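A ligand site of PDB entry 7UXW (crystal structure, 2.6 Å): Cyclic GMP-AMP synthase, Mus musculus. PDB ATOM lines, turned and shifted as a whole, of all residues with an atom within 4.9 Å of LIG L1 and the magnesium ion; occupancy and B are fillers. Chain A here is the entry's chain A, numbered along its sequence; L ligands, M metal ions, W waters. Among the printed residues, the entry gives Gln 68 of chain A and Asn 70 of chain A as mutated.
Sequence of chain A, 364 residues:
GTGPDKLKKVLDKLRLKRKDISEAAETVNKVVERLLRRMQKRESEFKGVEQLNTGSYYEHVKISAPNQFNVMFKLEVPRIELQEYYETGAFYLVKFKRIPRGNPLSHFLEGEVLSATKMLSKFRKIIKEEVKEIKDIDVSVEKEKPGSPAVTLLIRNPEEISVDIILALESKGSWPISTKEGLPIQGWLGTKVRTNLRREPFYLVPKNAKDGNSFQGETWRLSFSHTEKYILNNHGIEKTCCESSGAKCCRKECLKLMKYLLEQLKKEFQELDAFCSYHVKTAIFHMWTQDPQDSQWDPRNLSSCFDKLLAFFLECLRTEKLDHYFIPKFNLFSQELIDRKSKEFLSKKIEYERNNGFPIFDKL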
ATOM      1  N   GLY A  55      26.335 -13.985  -9.983  1.00  0.00           N
ATOM      2  CA  GLY A  55      25.522 -12.840  -9.631  1.00  0.00           C
ATOM      3  C   GLY A  55      24.881 -12.177 -10.827  1.00  0.00           C
ATOM      4  O   GLY A  55      24.896 -12.726 -11.933  1.00  0.00           O
ATOM      5  N   SER A  56      24.369 -10.962 -10.594  1.00  0.00           N
ATOM      6  CA  SER A  56      23.372 -10.347 -11.455  1.00  0.00           C
ATOM      7  C   SER A  56      23.913 -10.047 -12.841  1.00  0.00           C
ATOM      8  O   SER A  56      23.208 -10.242 -13.826  1.00  0.00           O
ATOM      9  CB  SER A  56      22.756  -9.085 -10.812  1.00  0.00           C
ATOM     10  OG  SER A  56      23.734  -8.148 -10.354  1.00  0.00           O
ATOM     11  N   GLU A  59      24.007 -13.099 -14.842  1.00  0.00           N
ATOM     12  CA  GLU A  59      22.641 -13.613 -14.981  1.00  0.00           C
ATOM     13  C   GLU A  59      21.763 -12.735 -15.882  1.00  0.00           C
ATOM     14  O   GLU A  59      20.633 -13.089 -16.190  1.00  0.00           O
ATOM     15  CB  GLU A  59      21.987 -13.742 -13.608  1.00  0.00           C
ATOM     16  CG  GLU A  59      22.619 -14.780 -12.691  1.00  0.00           C
ATOM     17  CD  GLU A  59      22.225 -14.582 -11.217  1.00  0.00           C
ATOM     18  OE1 GLU A  59      21.835 -13.464 -10.819  1.00  0.00           O
ATOM     19  OE2 GLU A  59      22.341 -15.558 -10.440  1.00  0.00           O
ATOM     20  N   LYS A  62      21.384  -7.534 -13.867  1.00  0.00           N
ATOM     21  CA  LYS A  62      21.984  -6.297 -13.385  1.00  0.00           C
ATOM     22  C   LYS A  62      21.215  -5.129 -13.965  1.00  0.00           C
ATOM     23  O   LYS A  62      20.934  -5.125 -15.143  1.00  0.00           O
ATOM     24  CB  LYS A  62      23.460  -6.194 -13.802  1.00  0.00           C
ATOM     25  CG  LYS A  62      24.207  -5.029 -13.150  1.00  0.00           C
ATOM     26  CD  LYS A  62      24.462  -5.287 -11.677  1.00  0.00           C
ATOM     27  CE  LYS A  62      25.107  -4.078 -11.028  1.00  0.00           C
ATOM     28  NZ  LYS A  62      24.202  -2.899 -10.950  1.00  0.00           N
ATOM     29  N   GLN A  68      28.616  -3.368 -10.387  1.00  0.00           N
ATOM     30  CA  GLN A  68      28.884  -4.368  -9.388  1.00  0.00           C
ATOM     31  C   GLN A  68      28.964  -5.731 -10.074  1.00  0.00           C
ATOM     32  O   GLN A  68      28.067  -6.088 -10.824  1.00  0.00           O
ATOM     33  CB  GLN A  68      27.821  -4.309  -8.278  1.00  0.00           C
ATOM     34  CG  GLN A  68      28.307  -4.851  -6.940  1.00  0.00           C
ATOM     35  CD  GLN A  68      27.926  -6.304  -6.709  1.00  0.00           C
ATOM     36  OE1 GLN A  68      27.474  -7.003  -7.598  1.00  0.00           O
ATOM     37  NE2 GLN A  68      28.093  -6.768  -5.483  1.00  0.00           N
ATOM     38  N   ASN A  70      30.300  -9.954  -9.484  1.00  0.00           N
ATOM     39  CA  ASN A  70      30.621 -11.006  -8.519  1.00  0.00           C
ATOM     40  C   ASN A  70      31.447 -12.121  -9.152  1.00  0.00           C
ATOM     41  O   ASN A  70      31.092 -12.628 -10.206  1.00  0.00           O
ATOM     42  CB  ASN A  70      29.346 -11.554  -7.900  1.00  0.00           C
ATOM     43  CG  ASN A  70      28.456 -10.452  -7.347  1.00  0.00           C
ATOM     44  OD1 ASN A  70      27.593  -9.925  -8.039  1.00  0.00           O
ATOM     45  ND2 ASN A  70      28.634 -10.130  -6.067  1.00  0.00           N
ATOM     46  N   ARG A 221      29.746 -20.739   5.122  1.00  0.00           N
ATOM     47  CA  ARG A 221      28.330 -20.723   4.651  1.00  0.00           C
ATOM     48  C   ARG A 221      28.257 -21.362   3.269  1.00  0.00           C
ATOM     49  O   ARG A 221      29.184 -21.126   2.458  1.00  0.00           O
ATOM     50  CB  ARG A 221      27.774 -19.289   4.588  1.00  0.00           C
ATOM     51  CG  ARG A 221      26.270 -19.203   4.368  1.00  0.00           C
ATOM     52  CD  ARG A 221      25.753 -17.771   4.391  1.00  0.00           C
ATOM     53  NE  ARG A 221      26.166 -17.021   3.207  1.00  0.00           N
ATOM     54  CZ  ARG A 221      26.119 -15.701   3.079  1.00  0.00           C
ATOM     55  NH1 ARG A 221      25.674 -14.935   4.060  1.00  0.00           N
ATOM     56  NH2 ARG A 221      26.534 -15.128   1.952  1.00  0.00           N
ATOM     57  N   LEU A 222      27.193 -22.123   2.995  1.00  0.00           N
ATOM     58  CA  LEU A 222      26.989 -22.714   1.667  1.00  0.00           C
ATOM     59  C   LEU A 222      26.737 -21.624   0.631  1.00  0.00           C
ATOM     60  O   LEU A 222      26.094 -20.628   0.923  1.00  0.00           O
ATOM     61  CB  LEU A 222      25.814 -23.709   1.667  1.00  0.00           C
ATOM     62  CG  LEU A 222      26.054 -24.990   2.447  1.00  0.00           C
ATOM     63  CD1 LEU A 222      24.778 -25.747   2.699  1.00  0.00           C
ATOM     64  CD2 LEU A 222      27.055 -25.862   1.699  1.00  0.00           C
ATOM     65  N   SER A 225      25.571 -20.217  -5.941  1.00  0.00           N
ATOM     66  CA  SER A 225      25.585 -19.168  -6.943  1.00  0.00           C
ATOM     67  C   SER A 225      25.659 -19.717  -8.343  1.00  0.00           C
ATOM     68  O   SER A 225      25.120 -19.131  -9.274  1.00  0.00           O
ATOM     69  CB  SER A 225      26.776 -18.239  -6.709  1.00  0.00           C
ATOM     70  OG  SER A 225      26.526 -17.411  -5.600  1.00  0.00           O
ATOM     71  N   GLU A 228      22.042 -21.037  -9.018  1.00  0.00           N
ATOM     72  CA  GLU A 228      21.181 -19.895  -9.257  1.00  0.00           C
ATOM     73  C   GLU A 228      21.399 -19.296 -10.652  1.00  0.00           C
ATOM     74  O   GLU A 228      20.442 -18.884 -11.308  1.00  0.00           O
ATOM     75  CB  GLU A 228      21.411 -18.847  -8.181  1.00  0.00           C
ATOM     76  CG  GLU A 228      21.052 -19.332  -6.773  1.00  0.00           C
ATOM     77  CD  GLU A 228      21.664 -18.473  -5.710  1.00  0.00           C
ATOM     78  OE1 GLU A 228      22.245 -17.429  -6.071  1.00  0.00           O
ATOM     79  OE2 GLU A 228      21.534 -18.847  -4.512  1.00  0.00           O
ATOM     80  N   LYS A 259      14.050  -5.802  -7.687  1.00  0.00           N
ATOM     81  CA  LYS A 259      15.396  -5.399  -7.280  1.00  0.00           C
ATOM     82  C   LYS A 259      15.511  -3.879  -7.181  1.00  0.00           C
ATOM     83  O   LYS A 259      16.114  -3.351  -6.245  1.00  0.00           O
ATOM     84  CB  LYS A 259      16.425  -5.886  -8.269  1.00  0.00           C
ATOM     85  CG  LYS A 259      16.812  -7.308  -8.078  1.00  0.00           C
ATOM     86  CD  LYS A 259      17.463  -7.840  -9.341  1.00  0.00           C
ATOM     87  CE  LYS A 259      18.819  -7.184  -9.594  1.00  0.00           C
ATOM     88  NZ  LYS A 259      19.858  -7.789  -8.717  1.00  0.00           N
ATOM     89  N   GLU A 263      16.428  -1.433  -4.166  1.00  0.00           N
ATOM     90  CA  GLU A 263      17.596  -0.562  -4.340  1.00  0.00           C
ATOM     91  C   GLU A 263      17.267   0.918  -4.080  1.00  0.00           C
ATOM     92  O   GLU A 263      17.998   1.612  -3.356  1.00  0.00           O
ATOM     93  CB  GLU A 263      18.203  -0.739  -5.745  1.00  0.00           C
ATOM     94  CG  GLU A 263      19.332  -1.754  -5.822  1.00  0.00           C
ATOM     95  CD  GLU A 263      20.028  -1.789  -7.182  1.00  0.00           C
ATOM     96  OE1 GLU A 263      20.476  -0.720  -7.661  1.00  0.00           O
ATOM     97  OE2 GLU A 263      20.133  -2.905  -7.770  1.00  0.00           O
ATOM     98  N   SER A 277      19.514  -7.838  -1.863  1.00  0.00           N
ATOM     99  CA  SER A 277      18.923  -8.314  -3.109  1.00  0.00           C
ATOM    100  C   SER A 277      18.691  -9.813  -3.072  1.00  0.00           C
ATOM    101  O   SER A 277      17.799 -10.318  -3.733  1.00  0.00           O
ATOM    102  CB  SER A 277      19.725  -7.866  -4.337  1.00  0.00           C
ATOM    103  OG  SER A 277      21.058  -8.277  -4.256  1.00  0.00           O
ATOM    104  N   TYR A 278      19.450 -10.537  -2.255  1.00  0.00           N
ATOM    105  CA  TYR A 278      19.322 -12.020  -2.193  1.00  0.00           C
ATOM    106  C   TYR A 278      17.935 -12.394  -1.668  1.00  0.00           C
ATOM    107  O   TYR A 278      17.429 -13.473  -2.034  1.00  0.00           O
ATOM    108  CB  TYR A 278      20.417 -12.658  -1.330  1.00  0.00           C
ATOM    109  CG  TYR A 278      20.450 -14.157  -1.499  1.00  0.00           C
ATOM    110  CD1 TYR A 278      20.829 -14.712  -2.708  1.00  0.00           C
ATOM    111  CD2 TYR A 278      20.042 -15.033  -0.497  1.00  0.00           C
ATOM    112  CE1 TYR A 278      20.857 -16.075  -2.907  1.00  0.00           C
ATOM    113  CE2 TYR A 278      20.066 -16.406  -0.686  1.00  0.00           C
ATOM    114  CZ  TYR A 278      20.465 -16.924  -1.902  1.00  0.00           C
ATOM    115  OH  TYR A 278      20.491 -18.265  -2.131  1.00  0.00           O
ATOM    116  N   LYS A 281      15.757 -12.241  -4.711  1.00  0.00           N
ATOM    117  CA  LYS A 281      16.122 -13.373  -5.577  1.00  0.00           C
ATOM    118  C   LYS A 281      15.493 -14.670  -5.065  1.00  0.00           C
ATOM    119  O   LYS A 281      14.923 -15.450  -5.829  1.00  0.00           O
ATOM    120  CB  LYS A 281      17.635 -13.531  -5.629  1.00  0.00           C
ATOM    121  CG  LYS A 281      18.132 -14.320  -6.816  1.00  0.00           C
ATOM    122  CD  LYS A 281      19.661 -14.372  -6.804  1.00  0.00           C
ATOM    123  CE  LYS A 281      20.187 -15.062  -8.036  1.00  0.00           C
ATOM    124  NZ  LYS A 281      21.623 -15.447  -7.910  1.00  0.00           N
ATOM    125  N   HIS A 324      15.268 -20.052   2.654  1.00  0.00           N
ATOM    126  CA  HIS A 324      16.321 -20.258   1.672  1.00  0.00           C
ATOM    127  C   HIS A 324      15.798 -21.306   0.698  1.00  0.00           C
ATOM    128  O   HIS A 324      15.275 -22.335   1.117  1.00  0.00           O
ATOM    129  CB  HIS A 324      17.579 -20.763   2.387  1.00  0.00           C
ATOM    130  CG  HIS A 324      18.843 -20.565   1.621  1.00  0.00           C
ATOM    131  ND1 HIS A 324      19.144 -21.280   0.490  1.00  0.00           N
ATOM    132  CD2 HIS A 324      19.904 -19.759   1.845  1.00  0.00           C
ATOM    133  CE1 HIS A 324      20.330 -20.925   0.048  1.00  0.00           C
ATOM    134  NE2 HIS A 324      20.816 -19.995   0.853  1.00  0.00           N
HETATM  135  P1  LIG L   1      23.031  -7.244  -7.297  1.00  0.00           P
HETATM  136  O1  LIG L   1      22.575  -6.649  -8.610  1.00  0.00           O
HETATM  137  O2  LIG L   1      24.535  -7.254  -7.177  1.00  0.00           O
HETATM  138  O3  LIG L   1      22.340  -6.617  -6.108  1.00  0.00           O
HETATM  139  P2  LIG L   1      23.397 -10.132  -7.039  1.00  0.00           P
HETATM  140  O4  LIG L   1      22.494 -11.316  -7.167  1.00  0.00           O
HETATM  141  O5  LIG L   1      24.635 -10.079  -7.862  1.00  0.00           O
HETATM  142  O6  LIG L   1      22.563  -8.791  -7.281  1.00  0.00           O
HETATM  143  P3  LIG L   1      25.133  -9.773  -4.693  1.00  0.00           P
HETATM  144  O7  LIG L   1      24.816  -9.155  -3.374  1.00  0.00           O
HETATM  145  O8  LIG L   1      26.088  -9.086  -5.624  1.00  0.00           O
HETATM  146  O9  LIG L   1      23.759  -9.946  -5.504  1.00  0.00           O
HETATM  147  O10 LIG L   1      25.592 -11.286  -4.422  1.00  0.00           O
HETATM  148  C1  LIG L   1      26.142 -12.124  -5.461  1.00  0.00           C
HETATM  149  C2  LIG L   1      25.625 -13.533  -5.299  1.00  0.00           C
HETATM  150  O11 LIG L   1      26.044 -14.078  -4.010  1.00  0.00           O
HETATM  151  C3  LIG L   1      24.100 -13.710  -5.273  1.00  0.00           C
HETATM  152  O12 LIG L   1      23.556 -13.711  -6.587  1.00  0.00           O
HETATM  153  C4  LIG L   1      23.970 -15.067  -4.574  1.00  0.00           C
HETATM  154  O13 LIG L   1      24.185 -16.144  -5.460  1.00  0.00           O
HETATM  155  C5  LIG L   1      25.068 -14.966  -3.518  1.00  0.00           C
HETATM  156  N1  LIG L   1      24.591 -14.464  -2.212  1.00  0.00           N
HETATM  157  C6  LIG L   1      24.484 -13.154  -1.813  1.00  0.00           C
HETATM  158  N2  LIG L   1      24.009 -13.040  -0.583  1.00  0.00           N
HETATM  159  C7  LIG L   1      23.792 -14.354  -0.168  1.00  0.00           C
HETATM  160  C8  LIG L   1      23.301 -14.902   1.030  1.00  0.00           C
HETATM  161  N3  LIG L   1      22.922 -14.175   2.069  1.00  0.00           N
HETATM  162  N4  LIG L   1      23.213 -16.251   1.108  1.00  0.00           N
HETATM  163  C9  LIG L   1      23.604 -16.981   0.050  1.00  0.00           C
HETATM  164  N5  LIG L   1      24.079 -16.574  -1.121  1.00  0.00           N
HETATM  165  C10 LIG L   1      24.152 -15.233  -1.172  1.00  0.00           C
HETATM  166  P1  LG2 L   2      24.793  -8.862   5.214  1.00  0.00           P
HETATM  167  O1  LG2 L   2      25.163  -7.783   4.230  1.00  0.00           O
HETATM  168  O2  LG2 L   2      23.965  -9.959   4.593  1.00  0.00           O
HETATM  169  O3  LG2 L   2      24.176  -8.317   6.482  1.00  0.00           O
HETATM  170  O4  LG2 L   2      26.170  -9.568   5.690  1.00  0.00           O
HETATM  171  P2  LG2 L   2      27.664  -9.574   5.102  1.00  0.00           P
HETATM  172  O5  LG2 L   2      27.884  -8.297   4.354  1.00  0.00           O
HETATM  173  O6  LG2 L   2      28.619  -9.985   6.172  1.00  0.00           O
HETATM  174  O7  LG2 L   2      27.564 -10.766   4.042  1.00  0.00           O
HETATM  175  P3  LG2 L   2      26.691 -10.948   2.702  1.00  0.00           P
HETATM  176  O8  LG2 L   2      25.972 -12.245   2.788  1.00  0.00           O
HETATM  177  O9  LG2 L   2      25.895  -9.707   2.463  1.00  0.00           O
HETATM  178  O10 LG2 L   2      27.866 -11.043   1.616  1.00  0.00           O
HETATM  179  C1  LG2 L   2      28.482  -9.827   1.142  1.00  0.00           C
HETATM  180  C2  LG2 L   2      28.704  -9.924  -0.344  1.00  0.00           C
HETATM  181  O11 LG2 L   2      29.598 -11.029  -0.614  1.00  0.00           O
HETATM  182  C3  LG2 L   2      27.470 -10.229  -1.199  1.00  0.00           C
HETATM  183  O12 LG2 L   2      26.692  -9.073  -1.488  1.00  0.00           O
HETATM  184  C4  LG2 L   2      28.130 -10.805  -2.451  1.00  0.00           C
HETATM  185  O13 LG2 L   2      28.677  -9.824  -3.302  1.00  0.00           O
HETATM  186  C5  LG2 L   2      29.222 -11.669  -1.814  1.00  0.00           C
HETATM  187  N1  LG2 L   2      28.773 -13.027  -1.531  1.00  0.00           N
HETATM  188  C6  LG2 L   2      28.307 -13.519  -0.340  1.00  0.00           C
HETATM  189  N2  LG2 L   2      27.975 -14.786  -0.393  1.00  0.00           N
HETATM  190  C7  LG2 L   2      28.229 -15.143  -1.716  1.00  0.00           C
HETATM  191  C8  LG2 L   2      28.054 -16.388  -2.374  1.00  0.00           C
HETATM  192  O14 LG2 L   2      27.611 -17.438  -1.894  1.00  0.00           O
HETATM  193  N3  LG2 L   2      28.431 -16.320  -3.715  1.00  0.00           N
HETATM  194  C9  LG2 L   2      28.911 -15.199  -4.350  1.00  0.00           C
HETATM  195  N4  LG2 L   2      29.215 -15.323  -5.643  1.00  0.00           N
HETATM  196  N5  LG2 L   2      29.075 -14.023  -3.736  1.00  0.00           N
HETATM  197  C10 LG2 L   2      28.717 -14.072  -2.422  1.00  0.00           C
HETATM  198 MG    MG M   1      26.018  -8.494  -7.683  1.00  0.00          MG
HETATM  199  O   HOH W   1      25.988  -8.025  -9.708  1.00  0.00           O
HETATM  200  O   HOH W   2      21.702  -4.543  -9.886  1.00  0.00           O
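The side-chain carboxylate (OE1) of Glu 228 sits at hydrogen-bond distance from an oxygen (O13) of LIG L1 (2.4 Å).
The backbone NH (N) of Ser 56 lies close to an oxygen (O5) of LIG L1 (2.9 Å).
OG of Ser 56 lies within hydrogen-bond range of O1 of LIG L1 (2.6 Å).
The side-chain hydroxyl of Ser 225 sits at hydrogen-bond distance from an oxygen (O13) of LIG L1 (2.7 Å).
The side-chain hydroxyl of Ser 277 is in hydrogen-bond range of an oxygen (O3) of LIG L1 (2.8 Å).
O12 of LIG L1 sits at hydrogen-bond distance from NZ of Lys 281, at 2.9 Å.
NZ of Lys 259 lies within salt-bridge range of O1 of LIG L1, 2.9 Å away.
The side-chain amide nitrogen of Asn 70 lies within hydrogen-bond range of an oxygen (O13) of LG2 L2, at 2.8 Å.
N3 of LG2 L2 lies within hydrogen-bond range of OG of Ser 225, 2.9 Å away.
NH1 of Arg 221 is in salt-bridge range of O8 of LG2 L2 (3.0 Å).
An oxygen (O7) of LIG L1 is in hydrogen-bond range of an oxygen (O12) of LG2 L2 (2.7 Å).
OE1 of Glu 228 is in salt-bridge range of NZ of Lys 281, at 2.8 Å.
The side-chain carboxylate (OE2) of Glu 228 sits at hydrogen-bond distance from the side-chain hydroxyl (OH) of Tyr 278 (2.7 Å).
O of Ser 56 lies within hydrogen-bond range of N of Lys 62 (3.3 Å).
The side-chain amino group of Lys 281 is in salt-bridge range of the side-chain carboxylate of Glu 59.
OH of Tyr 278 lies close to NE2 of His 324 (3.5 Å).
The guanidinium group of Arg 221 lies close to a nitrogen (N3) of LIG L1 (3.5 Å).
Merely in contact with LIG L1: Gly 55, Tyr 278 and Lys 62.
Hydrophobic or aromatic side chains that line LIG L1: Tyr 278.
12 residues have an atom within 4 Å of LIG L1: Gly 55, Ser 56, Lys 62, Gln 68, Asn 70, Arg 221, Ser 225, Glu 228, Lys 259, Ser 277, Tyr 278 and Lys 281.
The nearest printed residue that does not touch LIG L1 is His 324 (4.2 Å).
Merely in contact with the magnesium ion: Ser 56 (3.5 Å).
Of the 16 residues printed, 3 come within 4 Å of the magnesium ion.
The magnesium ion is bound by O2 of LIG L1 (2.0 Å), water W1 (2.1 Å), OE1 of Gln 68 (2.1 Å), O5 of LIG L1 (2.1 Å), O8 of LIG L1 (2.1 Å) and OD1 of Asn 70 (2.2 Å).
The magnesium ion has six donor atoms within binding distance.
Water W1 bridges the backbone carbonyl oxygen (O) of Gln 68 (3.1 Å) and the backbone NH (N) of Ser 56 (3.5 Å).
Water W2 lies within hydrogen-bond range of O1 of LIG L1 (2.6 Å), OE2 of Glu 263 (3.1 Å) and NZ of Lys 62 (3.2 Å).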
